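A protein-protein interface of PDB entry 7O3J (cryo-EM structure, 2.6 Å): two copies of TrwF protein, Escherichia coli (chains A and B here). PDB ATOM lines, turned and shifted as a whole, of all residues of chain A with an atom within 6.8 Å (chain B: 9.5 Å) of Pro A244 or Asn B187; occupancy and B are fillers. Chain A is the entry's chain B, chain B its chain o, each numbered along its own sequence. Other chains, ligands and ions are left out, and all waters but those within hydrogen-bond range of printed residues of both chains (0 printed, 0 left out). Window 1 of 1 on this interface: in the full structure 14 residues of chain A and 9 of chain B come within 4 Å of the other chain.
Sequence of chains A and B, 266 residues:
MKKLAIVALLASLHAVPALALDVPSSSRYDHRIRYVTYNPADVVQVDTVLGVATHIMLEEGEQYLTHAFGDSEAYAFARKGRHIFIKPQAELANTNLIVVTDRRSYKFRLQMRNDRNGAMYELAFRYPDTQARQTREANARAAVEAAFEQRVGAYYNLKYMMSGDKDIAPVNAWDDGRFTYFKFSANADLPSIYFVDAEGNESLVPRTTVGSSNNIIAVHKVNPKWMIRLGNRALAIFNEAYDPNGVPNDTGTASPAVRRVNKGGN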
ATOM      1  N   GLY A 177      -0.766 -23.479  23.230  1.00  0.00           N
ATOM      2  CA  GLY A 177      -1.797 -22.940  22.384  1.00  0.00           C
ATOM      3  C   GLY A 177      -1.292 -22.357  21.084  1.00  0.00           C
ATOM      4  O   GLY A 177      -2.080 -22.189  20.150  1.00  0.00           O
ATOM      5  N   ARG A 178      -0.006 -22.045  21.002  1.00  0.00           N
ATOM      6  CA  ARG A 178       0.594 -21.544  19.776  1.00  0.00           C
ATOM      7  C   ARG A 178       1.703 -22.444  19.265  1.00  0.00           C
ATOM      8  O   ARG A 178       1.738 -22.761  18.073  1.00  0.00           O
ATOM      9  CB  ARG A 178       1.124 -20.123  19.996  1.00  0.00           C
ATOM     10  CG  ARG A 178       1.820 -19.531  18.791  1.00  0.00           C
ATOM     11  CD  ARG A 178       1.543 -18.052  18.674  1.00  0.00           C
ATOM     12  NE  ARG A 178       0.134 -17.757  18.889  1.00  0.00           N
ATOM     13  CZ  ARG A 178      -0.315 -16.648  19.460  1.00  0.00           C
ATOM     14  NH1 ARG A 178       0.534 -15.723  19.875  1.00  0.00           N
ATOM     15  NH2 ARG A 178      -1.617 -16.466  19.618  1.00  0.00           N
ATOM     16  N   LYS A 221       3.520 -24.829  15.304  1.00  0.00           N
ATOM     17  CA  LYS A 221       2.164 -25.185  14.936  1.00  0.00           C
ATOM     18  C   LYS A 221       1.591 -26.045  16.050  1.00  0.00           C
ATOM     19  O   LYS A 221       2.332 -26.685  16.793  1.00  0.00           O
ATOM     20  CB  LYS A 221       2.155 -25.922  13.591  1.00  0.00           C
ATOM     21  CG  LYS A 221       0.797 -26.309  13.053  1.00  0.00           C
ATOM     22  CD  LYS A 221      -0.005 -25.086  12.672  1.00  0.00           C
ATOM     23  CE  LYS A 221      -1.373 -25.465  12.147  1.00  0.00           C
ATOM     24  NZ  LYS A 221      -1.290 -26.198  10.863  1.00  0.00           N
ATOM     25  N   VAL A 222       0.271 -26.041  16.175  1.00  0.00           N
ATOM     26  CA  VAL A 222      -0.440 -26.969  17.043  1.00  0.00           C
ATOM     27  C   VAL A 222      -1.264 -27.873  16.142  1.00  0.00           C
ATOM     28  O   VAL A 222      -2.030 -27.387  15.303  1.00  0.00           O
ATOM     29  CB  VAL A 222      -1.324 -26.247  18.068  1.00  0.00           C
ATOM     30  CG1 VAL A 222      -2.236 -27.227  18.750  1.00  0.00           C
ATOM     31  CG2 VAL A 222      -0.473 -25.551  19.087  1.00  0.00           C
ATOM     32  N   ASN A 223      -1.096 -29.178  16.301  1.00  0.00           N
ATOM     33  CA  ASN A 223      -1.623 -30.157  15.370  1.00  0.00           C
ATOM     34  C   ASN A 223      -2.093 -31.374  16.149  1.00  0.00           C
ATOM     35  O   ASN A 223      -1.556 -31.665  17.222  1.00  0.00           O
ATOM     36  CB  ASN A 223      -0.542 -30.549  14.351  1.00  0.00           C
ATOM     37  CG  ASN A 223      -1.063 -31.404  13.235  1.00  0.00           C
ATOM     38  OD1 ASN A 223      -1.966 -31.012  12.509  1.00  0.00           O
ATOM     39  ND2 ASN A 223      -0.471 -32.573  13.069  1.00  0.00           N
ATOM     40  N   ALA A 241      -6.133 -33.560  23.213  1.00  0.00           N
ATOM     41  CA  ALA A 241      -6.968 -32.435  23.608  1.00  0.00           C
ATOM     42  C   ALA A 241      -6.844 -31.317  22.591  1.00  0.00           C
ATOM     43  O   ALA A 241      -6.656 -30.149  22.930  1.00  0.00           O
ATOM     44  CB  ALA A 241      -6.602 -31.941  25.000  1.00  0.00           C
ATOM     45  N   TYR A 242      -6.945 -31.672  21.315  1.00  0.00           N
ATOM     46  CA  TYR A 242      -6.720 -30.706  20.251  1.00  0.00           C
ATOM     47  C   TYR A 242      -7.829 -29.667  20.221  1.00  0.00           C
ATOM     48  O   TYR A 242      -9.013 -30.004  20.170  1.00  0.00           O
ATOM     49  CB  TYR A 242      -6.632 -31.411  18.904  1.00  0.00           C
ATOM     50  CG  TYR A 242      -6.429 -30.466  17.751  1.00  0.00           C
ATOM     51  CD1 TYR A 242      -5.360 -29.594  17.730  1.00  0.00           C
ATOM     52  CD2 TYR A 242      -7.311 -30.444  16.689  1.00  0.00           C
ATOM     53  CE1 TYR A 242      -5.171 -28.729  16.683  1.00  0.00           C
ATOM     54  CE2 TYR A 242      -7.131 -29.581  15.636  1.00  0.00           C
ATOM     55  CZ  TYR A 242      -6.059 -28.727  15.639  1.00  0.00           C
ATOM     56  OH  TYR A 242      -5.872 -27.864  14.588  1.00  0.00           O
ATOM     57  N   ASP A 243      -7.437 -28.399  20.241  1.00  0.00           N
ATOM     58  CA  ASP A 243      -8.377 -27.291  20.146  1.00  0.00           C
ATOM     59  C   ASP A 243      -8.306 -26.694  18.751  1.00  0.00           C
ATOM     60  O   ASP A 243      -7.294 -26.067  18.406  1.00  0.00           O
ATOM     61  CB  ASP A 243      -8.064 -26.226  21.194  1.00  0.00           C
ATOM     62  CG  ASP A 243      -9.164 -25.204  21.325  1.00  0.00           C
ATOM     63  OD1 ASP A 243      -8.887 -24.097  21.828  1.00  0.00           O
ATOM     64  OD2 ASP A 243     -10.304 -25.504  20.918  1.00  0.00           O
ATOM     65  N   PRO A 244      -9.327 -26.873  17.915  1.00  0.00           N
ATOM     66  CA  PRO A 244      -9.286 -26.261  16.580  1.00  0.00           C
ATOM     67  C   PRO A 244      -9.217 -24.749  16.619  1.00  0.00           C
ATOM     68  O   PRO A 244      -8.562 -24.144  15.763  1.00  0.00           O
ATOM     69  CB  PRO A 244     -10.589 -26.748  15.934  1.00  0.00           C
ATOM     70  CG  PRO A 244     -11.012 -27.926  16.746  1.00  0.00           C
ATOM     71  CD  PRO A 244     -10.572 -27.621  18.135  1.00  0.00           C
ATOM     72  N   ASN A 245      -9.873 -24.117  17.591  1.00  0.00           N
ATOM     73  CA  ASN A 245      -9.932 -22.662  17.623  1.00  0.00           C
ATOM     74  C   ASN A 245      -8.576 -22.055  17.950  1.00  0.00           C
ATOM     75  O   ASN A 245      -8.108 -21.150  17.255  1.00  0.00           O
ATOM     76  CB  ASN A 245     -10.983 -22.210  18.631  1.00  0.00           C
ATOM     77  CG  ASN A 245     -12.340 -22.803  18.351  1.00  0.00           C
ATOM     78  OD1 ASN A 245     -12.603 -23.277  17.247  1.00  0.00           O
ATOM     79  ND2 ASN A 245     -13.208 -22.792  19.351  1.00  0.00           N
ATOM     80  N   GLY A 246      -7.929 -22.542  18.997  1.00  0.00           N
ATOM     81  CA  GLY A 246      -6.687 -21.922  19.395  1.00  0.00           C
ATOM     82  C   GLY A 246      -6.924 -20.518  19.924  1.00  0.00           C
ATOM     83  O   GLY A 246      -8.036 -20.132  20.288  1.00  0.00           O
ATOM     84  N   VAL A 247      -5.847 -19.742  19.954  1.00  0.00           N
ATOM     85  CA  VAL A 247      -5.926 -18.350  20.382  1.00  0.00           C
ATOM     86  C   VAL A 247      -5.388 -17.462  19.264  1.00  0.00           C
ATOM     87  O   VAL A 247      -4.307 -17.726  18.720  1.00  0.00           O
ATOM     88  CB  VAL A 247      -5.198 -18.137  21.722  1.00  0.00           C
ATOM     89  CG1 VAL A 247      -3.687 -18.297  21.580  1.00  0.00           C
ATOM     90  CG2 VAL A 247      -5.547 -16.776  22.301  1.00  0.00           C
ATOM     91  N   LYS B 166     -14.751 -31.560   6.478  1.00  0.00           N
ATOM     92  CA  LYS B 166     -15.005 -30.516   7.463  1.00  0.00           C
ATOM     93  C   LYS B 166     -13.766 -30.102   8.240  1.00  0.00           C
ATOM     94  O   LYS B 166     -13.834 -29.138   9.005  1.00  0.00           O
ATOM     95  CB  LYS B 166     -16.080 -30.971   8.443  1.00  0.00           C
ATOM     96  CG  LYS B 166     -17.340 -31.452   7.780  1.00  0.00           C
ATOM     97  CD  LYS B 166     -18.056 -30.324   7.091  1.00  0.00           C
ATOM     98  CE  LYS B 166     -19.283 -30.837   6.378  1.00  0.00           C
ATOM     99  NZ  LYS B 166     -20.285 -31.356   7.341  1.00  0.00           N
ATOM    100  N   ASP B 167     -12.652 -30.808   8.088  1.00  0.00           N
ATOM    101  CA  ASP B 167     -11.443 -30.435   8.807  1.00  0.00           C
ATOM    102  C   ASP B 167     -10.785 -29.178   8.254  1.00  0.00           C
ATOM    103  O   ASP B 167     -10.008 -28.540   8.969  1.00  0.00           O
ATOM    104  CB  ASP B 167     -10.461 -31.609   8.804  1.00  0.00           C
ATOM    105  CG  ASP B 167     -10.007 -31.993   7.411  1.00  0.00           C
ATOM    106  OD1 ASP B 167     -10.473 -31.386   6.432  1.00  0.00           O
ATOM    107  OD2 ASP B 167      -9.184 -32.918   7.293  1.00  0.00           O
ATOM    108  N   ILE B 168     -11.074 -28.808   7.011  1.00  0.00           N
ATOM    109  CA  ILE B 168     -10.573 -27.570   6.436  1.00  0.00           C
ATOM    110  C   ILE B 168     -11.669 -26.508   6.356  1.00  0.00           C
ATOM    111  O   ILE B 168     -11.540 -25.544   5.611  1.00  0.00           O
ATOM    112  CB  ILE B 168      -9.932 -27.805   5.061  1.00  0.00           C
ATOM    113  CG1 ILE B 168     -10.963 -28.337   4.069  1.00  0.00           C
ATOM    114  CG2 ILE B 168      -8.774 -28.764   5.173  1.00  0.00           C
ATOM    115  CD1 ILE B 168     -10.540 -28.199   2.643  1.00  0.00           C
ATOM    116  N   ALA B 169     -12.734 -26.668   7.116  1.00  0.00           N
ATOM    117  CA  ALA B 169     -13.887 -25.792   7.035  1.00  0.00           C
ATOM    118  C   ALA B 169     -13.641 -24.480   7.771  1.00  0.00           C
ATOM    119  O   ALA B 169     -12.905 -24.442   8.757  1.00  0.00           O
ATOM    120  CB  ALA B 169     -15.110 -26.478   7.622  1.00  0.00           C
ATOM    121  N   PRO B 170     -14.242 -23.389   7.304  1.00  0.00           N
ATOM    122  CA  PRO B 170     -14.202 -22.144   8.069  1.00  0.00           C
ATOM    123  C   PRO B 170     -15.144 -22.211   9.257  1.00  0.00           C
ATOM    124  O   PRO B 170     -16.082 -23.006   9.298  1.00  0.00           O
ATOM    125  CB  PRO B 170     -14.662 -21.086   7.061  1.00  0.00           C
ATOM    126  CG  PRO B 170     -14.809 -21.781   5.763  1.00  0.00           C
ATOM    127  CD  PRO B 170     -14.970 -23.226   6.041  1.00  0.00           C
ATOM    128  N   VAL B 171     -14.882 -21.352  10.240  1.00  0.00           N
ATOM    129  CA  VAL B 171     -15.786 -21.267  11.377  1.00  0.00           C
ATOM    130  C   VAL B 171     -16.953 -20.338  11.104  1.00  0.00           C
ATOM    131  O   VAL B 171     -17.975 -20.424  11.791  1.00  0.00           O
ATOM    132  CB  VAL B 171     -15.043 -20.821  12.647  1.00  0.00           C
ATOM    133  CG1 VAL B 171     -13.982 -21.829  13.006  1.00  0.00           C
ATOM    134  CG2 VAL B 171     -14.423 -19.463  12.451  1.00  0.00           C
ATOM    135  N   PHE B 184     -11.486 -18.291   9.412  1.00  0.00           N
ATOM    136  CA  PHE B 184     -10.863 -19.533   9.829  1.00  0.00           C
ATOM    137  C   PHE B 184     -10.277 -19.372  11.223  1.00  0.00           C
ATOM    138  O   PHE B 184      -9.931 -18.268  11.645  1.00  0.00           O
ATOM    139  CB  PHE B 184      -9.777 -19.958   8.845  1.00  0.00           C
ATOM    140  CG  PHE B 184     -10.294 -20.253   7.475  1.00  0.00           C
ATOM    141  CD1 PHE B 184     -10.417 -19.253   6.540  1.00  0.00           C
ATOM    142  CD2 PHE B 184     -10.669 -21.529   7.126  1.00  0.00           C
ATOM    143  CE1 PHE B 184     -10.898 -19.523   5.290  1.00  0.00           C
ATOM    144  CE2 PHE B 184     -11.151 -21.798   5.877  1.00  0.00           C
ATOM    145  CZ  PHE B 184     -11.265 -20.795   4.959  1.00  0.00           C
ATOM    146  N   SER B 185     -10.182 -20.484  11.943  1.00  0.00           N
ATOM    147  CA  SER B 185      -9.678 -20.442  13.304  1.00  0.00           C
ATOM    148  C   SER B 185      -8.168 -20.216  13.307  1.00  0.00           C
ATOM    149  O   SER B 185      -7.499 -20.256  12.274  1.00  0.00           O
ATOM    150  CB  SER B 185     -10.027 -21.728  14.042  1.00  0.00           C
ATOM    151  OG  SER B 185      -9.402 -22.838  13.436  1.00  0.00           O
ATOM    152  N   ALA B 186      -7.632 -19.967  14.502  1.00  0.00           N
ATOM    153  CA  ALA B 186      -6.213 -19.654  14.627  1.00  0.00           C
ATOM    154  C   ALA B 186      -5.341 -20.850  14.277  1.00  0.00           C
ATOM    155  O   ALA B 186      -4.278 -20.694  13.668  1.00  0.00           O
ATOM    156  CB  ALA B 186      -5.910 -19.168  16.040  1.00  0.00           C
ATOM    157  N   ASN B 187      -5.764 -22.048  14.660  1.00  0.00           N
ATOM    158  CA  ASN B 187      -4.960 -23.243  14.450  1.00  0.00           C
ATOM    159  C   ASN B 187      -5.147 -23.854  13.072  1.00  0.00           C
ATOM    160  O   ASN B 187      -4.486 -24.848  12.763  1.00  0.00           O
ATOM    161  CB  ASN B 187      -5.288 -24.285  15.516  1.00  0.00           C
ATOM    162  CG  ASN B 187      -4.647 -23.974  16.845  1.00  0.00           C
ATOM    163  OD1 ASN B 187      -3.737 -23.155  16.930  1.00  0.00           O
ATOM    164  ND2 ASN B 187      -5.120 -24.627  17.894  1.00  0.00           N
ATOM    165  N   ALA B 188      -6.016 -23.297  12.243  1.00  0.00           N
ATOM    166  CA  ALA B 188      -6.303 -23.866  10.937  1.00  0.00           C
ATOM    167  C   ALA B 188      -5.389 -23.275   9.877  1.00  0.00           C
ATOM    168  O   ALA B 188      -5.088 -22.080   9.899  1.00  0.00           O
ATOM    169  CB  ALA B 188      -7.760 -23.621  10.558  1.00  0.00           C
ATOM    170  N   ASP B 189      -4.940 -24.120   8.958  1.00  0.00           N
ATOM    171  CA  ASP B 189      -4.258 -23.630   7.774  1.00  0.00           C
ATOM    172  C   ASP B 189      -5.248 -22.902   6.878  1.00  0.00           C
ATOM    173  O   ASP B 189      -6.417 -23.277   6.781  1.00  0.00           O
ATOM    174  CB  ASP B 189      -3.628 -24.783   7.000  1.00  0.00           C
ATOM    175  CG  ASP B 189      -2.381 -25.318   7.660  1.00  0.00           C
ATOM    176  OD1 ASP B 189      -1.888 -24.686   8.611  1.00  0.00           O
ATOM    177  OD2 ASP B 189      -1.888 -26.375   7.222  1.00  0.00           O
ATOM    178  N   LEU B 190      -4.783 -21.848   6.226  1.00  0.00           N
ATOM    179  CA  LEU B 190      -5.635 -21.156   5.271  1.00  0.00           C
ATOM    180  C   LEU B 190      -5.663 -21.929   3.960  1.00  0.00           C
ATOM    181  O   LEU B 190      -4.609 -22.139   3.356  1.00  0.00           O
ATOM    182  CB  LEU B 190      -5.161 -19.735   5.026  1.00  0.00           C
ATOM    183  CG  LEU B 190      -5.367 -18.748   6.164  1.00  0.00           C
ATOM    184  CD1 LEU B 190      -4.911 -17.383   5.724  1.00  0.00           C
ATOM    185  CD2 LEU B 190      -6.810 -18.718   6.600  1.00  0.00           C
ATOM    186  N   SER B 213      -6.059 -10.777  12.844  1.00  0.00           N
ATOM    187  CA  SER B 213      -5.050 -11.824  12.855  1.00  0.00           C
ATOM    188  C   SER B 213      -4.949 -12.554  11.523  1.00  0.00           C
ATOM    189  O   SER B 213      -4.512 -13.706  11.487  1.00  0.00           O
ATOM    190  CB  SER B 213      -5.337 -12.811  13.985  1.00  0.00           C
ATOM    191  OG  SER B 213      -6.676 -13.254  13.945  1.00  0.00           O
ATOM    192  N   ASN B 215      -7.206 -13.848   9.759  1.00  0.00           N
ATOM    193  CA  ASN B 215      -8.009 -15.057   9.825  1.00  0.00           C
ATOM    194  C   ASN B 215      -9.197 -15.053   8.877  1.00  0.00           C
ATOM    195  O   ASN B 215      -9.956 -16.023   8.864  1.00  0.00           O
ATOM    196  CB  ASN B 215      -8.492 -15.287  11.257  1.00  0.00           C
ATOM    197  CG  ASN B 215      -9.246 -14.109  11.811  1.00  0.00           C
ATOM    198  OD1 ASN B 215      -9.455 -13.115  11.129  1.00  0.00           O
ATOM    199  ND2 ASN B 215      -9.679 -14.223  13.051  1.00  0.00           N
ATOM    200  N   LEU B 230      -7.512 -27.907   0.186  1.00  0.00           N
ATOM    201  CA  LEU B 230      -6.216 -27.843   0.851  1.00  0.00           C
ATOM    202  C   LEU B 230      -5.578 -29.216   0.740  1.00  0.00           C
ATOM    203  O   LEU B 230      -5.991 -30.148   1.432  1.00  0.00           O
ATOM    204  CB  LEU B 230      -6.349 -27.422   2.311  1.00  0.00           C
ATOM    205  CG  LEU B 230      -5.037 -27.275   3.078  1.00  0.00           C
ATOM    206  CD1 LEU B 230      -4.035 -26.467   2.291  1.00  0.00           C
ATOM    207  CD2 LEU B 230      -5.290 -26.635   4.409  1.00  0.00           C
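The backbone NH of Ala B186 sits at hydrogen-bond distance from the backbone carbonyl oxygen of Asn A245, 3.0 Å away.
The side-chain hydroxyl (OG) of Ser B185 lies within hydrogen-bond range of the backbone carbonyl oxygen (O) of Pro A244 (2.8 Å).
The side-chain amino group (NZ) of Lys A221 lies within salt-bridge range of the side-chain carboxylate (OD1) of Asp B189.
O of Asp A243 is in hydrogen-bond range of ND2 of Asn B187, 2.7 Å away.
OD1 of Asp A243 sits at hydrogen-bond distance from N of Gly A246 (3.4 Å).
The backbone carbonyl oxygen (O) of Val A247 lies within hydrogen-bond range of the guanidinium group (NH2) of Arg A178, 3.1 Å away.
Gly A177 touches Asn B187 (O to OD1, 3.7 Å).
Lys A221 touches Asn B187 (CE to O, 3.2 Å).
Asn B187 touches Val A222 (ND2 to CG1, 3.98 Å).
OH of Tyr A242 touches CB of Asn B187 (3.7 Å).
Pro A244 touches Asn B187 (O to CB, 3.3 Å).
Asn A245 touches Ser B185 (CA to CB, 3.7 Å).
Asn A245 touches Asn B187.
Gly A246 touches Asn B187.
O of Val A247 touches CB of Ala B186, 3.4 Å away.
Of chain B, only Ser B185 (2.8 Å) and Asn B187 (3.3 Å) come within 4 Å of Pro A244.
Asn B187 touches eight residues of chain A.
Printed residues of chain B within 4 Å of Val A222: Asn B187.
Printed residues of chain B within 4 Å of Gly A246: Asn B187 (3.5 Å).
Printed residues of chain A within 4 Å of Asp B189: Lys A221.
Of the printed residues of chain A, Ser B185 touches Pro A244 and Asn A245.
Val B171 touches none of the printed residues of chain A.
The nearest residue of chain A that does not touch Asn B187 is Val A247 (5.0 Å).
The nearest printed residue of chain B that does not touch Val A247 is Asn B187 (5.0 Å).
Of the 12 printed residues of chain A, 9 touch a printed residue of chain B.
Hydrophobic or aromatic side chains of chain A that line the printed part of chain B: Val A222 and Tyr A242.
Of the 16 printed residues of chain B, 4 touch a printed residue of chain A.
Hydrophobic or aromatic side chains of chain B within 4 Å of the printed part of chain A: Ala B186.
Along chain B the printed residues that touch a printed residue of chain A span positions 185 to 189.
Among the printed residues, Asp or Glu carboxylates within 4 Å of a Lys or Arg side-chain nitrogen of the other chain: Lys A221 with Asp B189 (2.8 Å).
No position is printed for both chains.
Of the 13 pairs that touch across the chains among the printed residues, none has its exchanged pair printed and touching as well.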
